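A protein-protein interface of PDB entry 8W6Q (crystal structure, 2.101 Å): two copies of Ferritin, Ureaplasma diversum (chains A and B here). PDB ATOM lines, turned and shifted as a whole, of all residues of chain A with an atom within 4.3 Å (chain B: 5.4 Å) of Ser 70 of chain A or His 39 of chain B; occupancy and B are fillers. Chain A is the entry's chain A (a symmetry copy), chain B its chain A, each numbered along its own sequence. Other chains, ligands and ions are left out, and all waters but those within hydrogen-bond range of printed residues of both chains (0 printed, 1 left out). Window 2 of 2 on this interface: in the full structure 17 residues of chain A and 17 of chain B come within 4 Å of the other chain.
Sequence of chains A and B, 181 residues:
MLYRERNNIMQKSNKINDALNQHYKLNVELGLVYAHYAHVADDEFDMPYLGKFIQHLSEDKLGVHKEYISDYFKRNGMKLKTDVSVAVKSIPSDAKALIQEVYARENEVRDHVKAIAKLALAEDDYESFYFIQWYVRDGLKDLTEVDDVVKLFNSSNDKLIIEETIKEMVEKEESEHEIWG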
ATOM      1  N   LYS A  66     -34.077 -18.682  -3.355  1.00  0.00           N
ATOM      2  CA  LYS A  66     -33.398 -19.690  -4.158  1.00  0.00           C
ATOM      3  C   LYS A  66     -31.892 -19.490  -4.124  1.00  0.00           C
ATOM      4  O   LYS A  66     -31.134 -20.468  -4.132  1.00  0.00           O
ATOM      5  CB  LYS A  66     -33.910 -19.684  -5.611  1.00  0.00           C
ATOM      6  CG  LYS A  66     -33.264 -18.654  -6.575  1.00  0.00           C
ATOM      7  CD  LYS A  66     -33.923 -18.712  -7.953  1.00  0.00           C
ATOM      8  CE  LYS A  66     -33.027 -18.126  -9.048  1.00  0.00           C
ATOM      9  NZ  LYS A  66     -32.593 -16.739  -8.708  1.00  0.00           N
ATOM     10  N   GLU A  67     -31.438 -18.263  -4.013  1.00  0.00           N
ATOM     11  CA  GLU A  67     -30.028 -17.975  -4.055  1.00  0.00           C
ATOM     12  C   GLU A  67     -29.265 -18.638  -2.943  1.00  0.00           C
ATOM     13  O   GLU A  67     -28.229 -19.212  -3.166  1.00  0.00           O
ATOM     14  CB  GLU A  67     -29.819 -16.472  -4.076  1.00  0.00           C
ATOM     15  CG  GLU A  67     -28.595 -15.898  -3.391  1.00  0.00           C
ATOM     16  CD  GLU A  67     -28.686 -14.389  -3.226  1.00  0.00           C
ATOM     17  OE1 GLU A  67     -29.588 -13.773  -3.834  1.00  0.00           O
ATOM     18  OE2 GLU A  67     -27.857 -13.821  -2.486  1.00  0.00           O
ATOM     19  N   TYR A  68     -29.804 -18.568  -1.747  1.00  0.00           N
ATOM     20  CA  TYR A  68     -29.091 -19.155  -0.619  1.00  0.00           C
ATOM     21  C   TYR A  68     -28.919 -20.660  -0.778  1.00  0.00           C
ATOM     22  O   TYR A  68     -27.909 -21.218  -0.326  1.00  0.00           O
ATOM     23  CB  TYR A  68     -29.817 -18.844   0.685  1.00  0.00           C
ATOM     24  CG  TYR A  68     -29.713 -17.400   1.105  1.00  0.00           C
ATOM     25  CD1 TYR A  68     -28.663 -16.603   0.669  1.00  0.00           C
ATOM     26  CD2 TYR A  68     -30.665 -16.834   1.933  1.00  0.00           C
ATOM     27  CE1 TYR A  68     -28.564 -15.269   1.055  1.00  0.00           C
ATOM     28  CE2 TYR A  68     -30.579 -15.504   2.329  1.00  0.00           C
ATOM     29  CZ  TYR A  68     -29.529 -14.731   1.883  1.00  0.00           C
ATOM     30  OH  TYR A  68     -29.444 -13.416   2.274  1.00  0.00           O
ATOM     31  N   ILE A  69     -29.896 -21.335  -1.396  1.00  0.00           N
ATOM     32  CA  ILE A  69     -29.773 -22.771  -1.618  1.00  0.00           C
ATOM     33  C   ILE A  69     -28.654 -23.053  -2.610  1.00  0.00           C
ATOM     34  O   ILE A  69     -27.802 -23.919  -2.380  1.00  0.00           O
ATOM     35  CB  ILE A  69     -31.117 -23.372  -2.081  1.00  0.00           C
ATOM     36  CG1 ILE A  69     -32.116 -23.361  -0.921  1.00  0.00           C
ATOM     37  CG2 ILE A  69     -30.937 -24.800  -2.589  1.00  0.00           C
ATOM     38  CD1 ILE A  69     -33.514 -23.790  -1.302  1.00  0.00           C
ATOM     39  N   SER A  70     -28.617 -22.300  -3.715  1.00  0.00           N
ATOM     40  CA  SER A  70     -27.544 -22.491  -4.684  1.00  0.00           C
ATOM     41  C   SER A  70     -26.188 -22.243  -4.035  1.00  0.00           C
ATOM     42  O   SER A  70     -25.242 -23.017  -4.232  1.00  0.00           O
ATOM     43  CB  SER A  70     -27.743 -21.570  -5.889  1.00  0.00           C
ATOM     44  OG  SER A  70     -26.491 -21.296  -6.516  1.00  0.00           O
ATOM     45  N   ASP A  71     -26.085 -21.183  -3.232  1.00  0.00           N
ATOM     46  CA  ASP A  71     -24.840 -20.877  -2.530  1.00  0.00           C
ATOM     47  C   ASP A  71     -24.453 -21.986  -1.556  1.00  0.00           C
ATOM     48  O   ASP A  71     -23.279 -22.359  -1.465  1.00  0.00           O
ATOM     49  CB  ASP A  71     -24.989 -19.544  -1.793  1.00  0.00           C
ATOM     50  CG  ASP A  71     -23.793 -19.212  -0.938  1.00  0.00           C
ATOM     51  OD1 ASP A  71     -22.761 -18.783  -1.507  1.00  0.00           O
ATOM     52  OD2 ASP A  71     -23.874 -19.414   0.296  1.00  0.00           O
ATOM     53  N   TYR A  72     -25.424 -22.510  -0.808  1.00  0.00           N
ATOM     54  CA  TYR A  72     -25.160 -23.617   0.103  1.00  0.00           C
ATOM     55  C   TYR A  72     -24.588 -24.824  -0.640  1.00  0.00           C
ATOM     56  O   TYR A  72     -23.597 -25.424  -0.200  1.00  0.00           O
ATOM     57  CB  TYR A  72     -26.459 -23.999   0.821  1.00  0.00           C
ATOM     58  CG  TYR A  72     -26.312 -25.077   1.874  1.00  0.00           C
ATOM     59  CD1 TYR A  72     -25.270 -25.042   2.786  1.00  0.00           C
ATOM     60  CD2 TYR A  72     -27.216 -26.131   1.956  1.00  0.00           C
ATOM     61  CE1 TYR A  72     -25.132 -26.022   3.762  1.00  0.00           C
ATOM     62  CE2 TYR A  72     -27.086 -27.114   2.932  1.00  0.00           C
ATOM     63  CZ  TYR A  72     -26.037 -27.047   3.835  1.00  0.00           C
ATOM     64  OH  TYR A  72     -25.873 -28.017   4.807  1.00  0.00           O
ATOM     65  N   PHE A  73     -25.183 -25.175  -1.785  1.00  0.00           N
ATOM     66  CA  PHE A  73     -24.752 -26.357  -2.529  1.00  0.00           C
ATOM     67  C   PHE A  73     -23.284 -26.255  -2.944  1.00  0.00           C
ATOM     68  O   PHE A  73     -22.544 -27.245  -2.884  1.00  0.00           O
ATOM     69  CB  PHE A  73     -25.642 -26.561  -3.756  1.00  0.00           C
ATOM     70  CG  PHE A  73     -27.007 -27.145  -3.452  1.00  0.00           C
ATOM     71  CD1 PHE A  73     -27.402 -27.429  -2.149  1.00  0.00           C
ATOM     72  CD2 PHE A  73     -27.895 -27.416  -4.488  1.00  0.00           C
ATOM     73  CE1 PHE A  73     -28.648 -27.980  -1.888  1.00  0.00           C
ATOM     74  CE2 PHE A  73     -29.142 -27.973  -4.239  1.00  0.00           C
ATOM     75  CZ  PHE A  73     -29.520 -28.258  -2.934  1.00  0.00           C
ATOM     76  N   LYS A  74     -22.844 -25.063  -3.363  1.00  0.00           N
ATOM     77  CA  LYS A  74     -21.449 -24.858  -3.735  1.00  0.00           C
ATOM     78  C   LYS A  74     -20.496 -25.093  -2.580  1.00  0.00           C
ATOM     79  O   LYS A  74     -19.317 -25.371  -2.810  1.00  0.00           O
ATOM     80  CB  LYS A  74     -21.216 -23.432  -4.239  1.00  0.00           C
ATOM     81  CG  LYS A  74     -22.042 -23.062  -5.455  1.00  0.00           C
ATOM     82  CD  LYS A  74     -21.547 -21.750  -6.058  1.00  0.00           C
ATOM     83  CE  LYS A  74     -22.597 -20.672  -6.051  1.00  0.00           C
ATOM     84  NZ  LYS A  74     -21.980 -19.385  -6.499  1.00  0.00           N
ATOM     85  N   LEU A  80     -26.950 -28.975  -7.740  1.00  0.00           N
ATOM     86  CA  LEU A  80     -28.134 -28.192  -8.086  1.00  0.00           C
ATOM     87  C   LEU A  80     -28.872 -28.821  -9.267  1.00  0.00           C
ATOM     88  O   LEU A  80     -28.253 -29.238 -10.250  1.00  0.00           O
ATOM     89  CB  LEU A  80     -27.750 -26.754  -8.430  1.00  0.00           C
ATOM     90  CG  LEU A  80     -28.930 -25.858  -8.834  1.00  0.00           C
ATOM     91  CD1 LEU A  80     -29.804 -25.560  -7.630  1.00  0.00           C
ATOM     92  CD2 LEU A  80     -28.450 -24.564  -9.495  1.00  0.00           C
ATOM     93  N   TYR B  34     -29.792 -19.309 -17.065  1.00  0.00           N
ATOM     94  CA  TYR B  34     -28.608 -18.542 -16.692  1.00  0.00           C
ATOM     95  C   TYR B  34     -28.311 -18.666 -15.204  1.00  0.00           C
ATOM     96  O   TYR B  34     -27.142 -18.685 -14.810  1.00  0.00           O
ATOM     97  CB  TYR B  34     -28.776 -17.077 -17.081  1.00  0.00           C
ATOM     98  CG  TYR B  34     -28.712 -16.810 -18.561  1.00  0.00           C
ATOM     99  CD1 TYR B  34     -28.324 -17.799 -19.454  1.00  0.00           C
ATOM    100  CD2 TYR B  34     -29.030 -15.558 -19.068  1.00  0.00           C
ATOM    101  CE1 TYR B  34     -28.270 -17.547 -20.819  1.00  0.00           C
ATOM    102  CE2 TYR B  34     -28.966 -15.295 -20.427  1.00  0.00           C
ATOM    103  CZ  TYR B  34     -28.579 -16.292 -21.292  1.00  0.00           C
ATOM    104  OH  TYR B  34     -28.528 -16.036 -22.642  1.00  0.00           O
ATOM    105  N   ALA B  35     -29.346 -18.750 -14.360  1.00  0.00           N
ATOM    106  CA  ALA B  35     -29.092 -18.942 -12.937  1.00  0.00           C
ATOM    107  C   ALA B  35     -28.373 -20.263 -12.704  1.00  0.00           C
ATOM    108  O   ALA B  35     -27.480 -20.355 -11.857  1.00  0.00           O
ATOM    109  CB  ALA B  35     -30.397 -18.898 -12.139  1.00  0.00           C
ATOM    110  N   HIS B  36     -28.747 -21.298 -13.461  1.00  0.00           N
ATOM    111  CA  HIS B  36     -28.051 -22.576 -13.351  1.00  0.00           C
ATOM    112  C   HIS B  36     -26.629 -22.471 -13.886  1.00  0.00           C
ATOM    113  O   HIS B  36     -25.676 -22.901 -13.226  1.00  0.00           O
ATOM    114  CB  HIS B  36     -28.818 -23.657 -14.100  1.00  0.00           C
ATOM    115  CG  HIS B  36     -28.438 -25.037 -13.685  1.00  0.00           C
ATOM    116  ND1 HIS B  36     -27.304 -25.667 -14.157  1.00  0.00           N
ATOM    117  CD2 HIS B  36     -29.021 -25.902 -12.825  1.00  0.00           C
ATOM    118  CE1 HIS B  36     -27.213 -26.867 -13.611  1.00  0.00           C
ATOM    119  NE2 HIS B  36     -28.243 -27.035 -12.800  1.00  0.00           N
ATOM    120  N   TYR B  37     -26.468 -21.877 -15.074  1.00  0.00           N
ATOM    121  CA  TYR B  37     -25.135 -21.701 -15.647  1.00  0.00           C
ATOM    122  C   TYR B  37     -24.230 -20.909 -14.717  1.00  0.00           C
ATOM    123  O   TYR B  37     -23.025 -21.176 -14.643  1.00  0.00           O
ATOM    124  CB  TYR B  37     -25.228 -21.006 -17.005  1.00  0.00           C
ATOM    125  CG  TYR B  37     -25.724 -21.863 -18.151  1.00  0.00           C
ATOM    126  CD1 TYR B  37     -26.158 -23.170 -17.948  1.00  0.00           C
ATOM    127  CD2 TYR B  37     -25.775 -21.351 -19.445  1.00  0.00           C
ATOM    128  CE1 TYR B  37     -26.612 -23.948 -19.010  1.00  0.00           C
ATOM    129  CE2 TYR B  37     -26.221 -22.114 -20.503  1.00  0.00           C
ATOM    130  CZ  TYR B  37     -26.637 -23.408 -20.283  1.00  0.00           C
ATOM    131  OH  TYR B  37     -27.088 -24.137 -21.350  1.00  0.00           O
ATOM    132  N   ALA B  38     -24.786 -19.920 -14.006  1.00  0.00           N
ATOM    133  CA  ALA B  38     -23.987 -19.153 -13.053  1.00  0.00           C
ATOM    134  C   ALA B  38     -23.489 -20.034 -11.917  1.00  0.00           C
ATOM    135  O   ALA B  38     -22.321 -19.949 -11.515  1.00  0.00           O
ATOM    136  CB  ALA B  38     -24.794 -17.983 -12.485  1.00  0.00           C
ATOM    137  N   HIS B  39     -24.372 -20.870 -11.369  1.00  0.00           N
ATOM    138  CA  HIS B  39     -23.964 -21.823 -10.341  1.00  0.00           C
ATOM    139  C   HIS B  39     -22.825 -22.711 -10.837  1.00  0.00           C
ATOM    140  O   HIS B  39     -21.806 -22.875 -10.158  1.00  0.00           O
ATOM    141  CB  HIS B  39     -25.168 -22.670  -9.919  1.00  0.00           C
ATOM    142  CG  HIS B  39     -24.844 -23.738  -8.921  1.00  0.00           C
ATOM    143  ND1 HIS B  39     -24.947 -23.546  -7.562  1.00  0.00           N
ATOM    144  CD2 HIS B  39     -24.412 -25.009  -9.088  1.00  0.00           C
ATOM    145  CE1 HIS B  39     -24.605 -24.656  -6.934  1.00  0.00           C
ATOM    146  NE2 HIS B  39     -24.267 -25.556  -7.838  1.00  0.00           N
ATOM    147  N   VAL B  40     -22.972 -23.262 -12.042  1.00  0.00           N
ATOM    148  CA  VAL B  40     -21.982 -24.183 -12.598  1.00  0.00           C
ATOM    149  C   VAL B  40     -20.649 -23.481 -12.868  1.00  0.00           C
ATOM    150  O   VAL B  40     -19.576 -24.065 -12.667  1.00  0.00           O
ATOM    151  CB  VAL B  40     -22.558 -24.819 -13.876  1.00  0.00           C
ATOM    152  CG1 VAL B  40     -21.478 -25.531 -14.671  1.00  0.00           C
ATOM    153  CG2 VAL B  40     -23.695 -25.774 -13.515  1.00  0.00           C
ATOM    154  N   ALA B  41     -20.690 -22.248 -13.387  1.00  0.00           N
ATOM    155  CA  ALA B  41     -19.454 -21.516 -13.648  1.00  0.00           C
ATOM    156  C   ALA B  41     -18.596 -21.422 -12.390  1.00  0.00           C
ATOM    157  O   ALA B  41     -17.383 -21.635 -12.434  1.00  0.00           O
ATOM    158  CB  ALA B  41     -19.774 -20.114 -14.184  1.00  0.00           C
ATOM    159  N   ASP B  42     -19.213 -21.102 -11.258  1.00  0.00           N
ATOM    160  CA  ASP B  42     -18.475 -21.070 -10.009  1.00  0.00           C
ATOM    161  C   ASP B  42     -18.168 -22.480  -9.541  1.00  0.00           C
ATOM    162  O   ASP B  42     -17.004 -22.845  -9.348  1.00  0.00           O
ATOM    163  CB  ASP B  42     -19.277 -20.314  -8.947  1.00  0.00           C
ATOM    164  CG  ASP B  42     -18.495 -20.078  -7.667  1.00  0.00           C
ATOM    165  OD1 ASP B  42     -17.299 -20.438  -7.609  1.00  0.00           O
ATOM    166  OD2 ASP B  42     -19.074 -19.501  -6.730  1.00  0.00           O
ATOM    167  N   ASP B  43     -19.204 -23.298  -9.398  1.00  0.00           N
ATOM    168  CA  ASP B  43     -19.069 -24.545  -8.657  1.00  0.00           C
ATOM    169  C   ASP B  43     -18.230 -25.569  -9.415  1.00  0.00           C
ATOM    170  O   ASP B  43     -17.380 -26.245  -8.824  1.00  0.00           O
ATOM    171  CB  ASP B  43     -20.448 -25.109  -8.354  1.00  0.00           C
ATOM    172  CG  ASP B  43     -20.379 -26.419  -7.629  1.00  0.00           C
ATOM    173  OD1 ASP B  43     -19.773 -26.438  -6.534  1.00  0.00           O
ATOM    174  OD2 ASP B  43     -20.916 -27.413  -8.164  1.00  0.00           O
ATOM    175  N   GLU B  44     -18.462 -25.717 -10.718  1.00  0.00           N
ATOM    176  CA  GLU B  44     -17.733 -26.728 -11.471  1.00  0.00           C
ATOM    177  C   GLU B  44     -16.497 -26.187 -12.179  1.00  0.00           C
ATOM    178  O   GLU B  44     -15.480 -26.876 -12.234  1.00  0.00           O
ATOM    179  CB  GLU B  44     -18.657 -27.402 -12.489  1.00  0.00           C
ATOM    180  CG  GLU B  44     -19.132 -28.789 -12.039  1.00  0.00           C
ATOM    181  CD  GLU B  44     -20.168 -29.397 -12.972  1.00  0.00           C
ATOM    182  OE1 GLU B  44     -19.783 -29.824 -14.084  1.00  0.00           O
ATOM    183  OE2 GLU B  44     -21.366 -29.438 -12.596  1.00  0.00           O
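OD2 of Asp 42 of chain B lies within salt-bridge range of NZ of Lys 74 of chain A (2.9 Å).
A ring nitrogen (ND1) of His 39 of chain B sits at hydrogen-bond distance from the side-chain hydroxyl (OG) of Ser 70 of chain A (2.9 Å).
A ring nitrogen (NE2) of His 36 of chain B lies within hydrogen-bond range of the backbone carbonyl oxygen (O) of Leu 80 of chain A, 3.4 Å away.
Among the printed residues, merely in contact across the chains: Lys 74 of chain A with His 39 of chain B (3.4 Å), Lys 74 of chain A with Asp 43 of chain B (3.6 Å), Leu 80 of chain A with His 39 of chain B (3.7 Å) and Phe 73 of chain A with His 39 of chain B (3.8 Å).
Ser 70 of chain A touches just one residue of chain B: His 39 (2.9 Å).
Of the printed residues of chain A, His 39 of chain B touches Ser 70, Phe 73, Lys 74 and Leu 80.
Of the printed residues of chain B, Phe 73 of chain A touches His 39.
Of the printed residues of chain A, His 36 of chain B touches Leu 80.
Printed residues of chain A within 4 Å of Asp 42 of chain B: Lys 74.
Of the printed residues of chain B, Leu 80 of chain A touches His 36 (3.4 Å) and His 39 (3.7 Å).
Hydrophobic or aromatic side chains of chain B that line the printed part of chain A: His 36 and His 39.
Hydrophobic or aromatic side chains of chain A within 4 Å of the printed part of chain B: Phe 73 and Leu 80.
Among the printed residues, Asp or Glu carboxylates within 4 Å of a Lys or Arg side-chain nitrogen of the other chain: Lys 74 of chain A with Asp 42 of chain B (2.9 Å).
No position is printed for both chains.
Of the 7 pairs that touch across the chains among the printed residues, none has its exchanged pair printed and touching as well.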
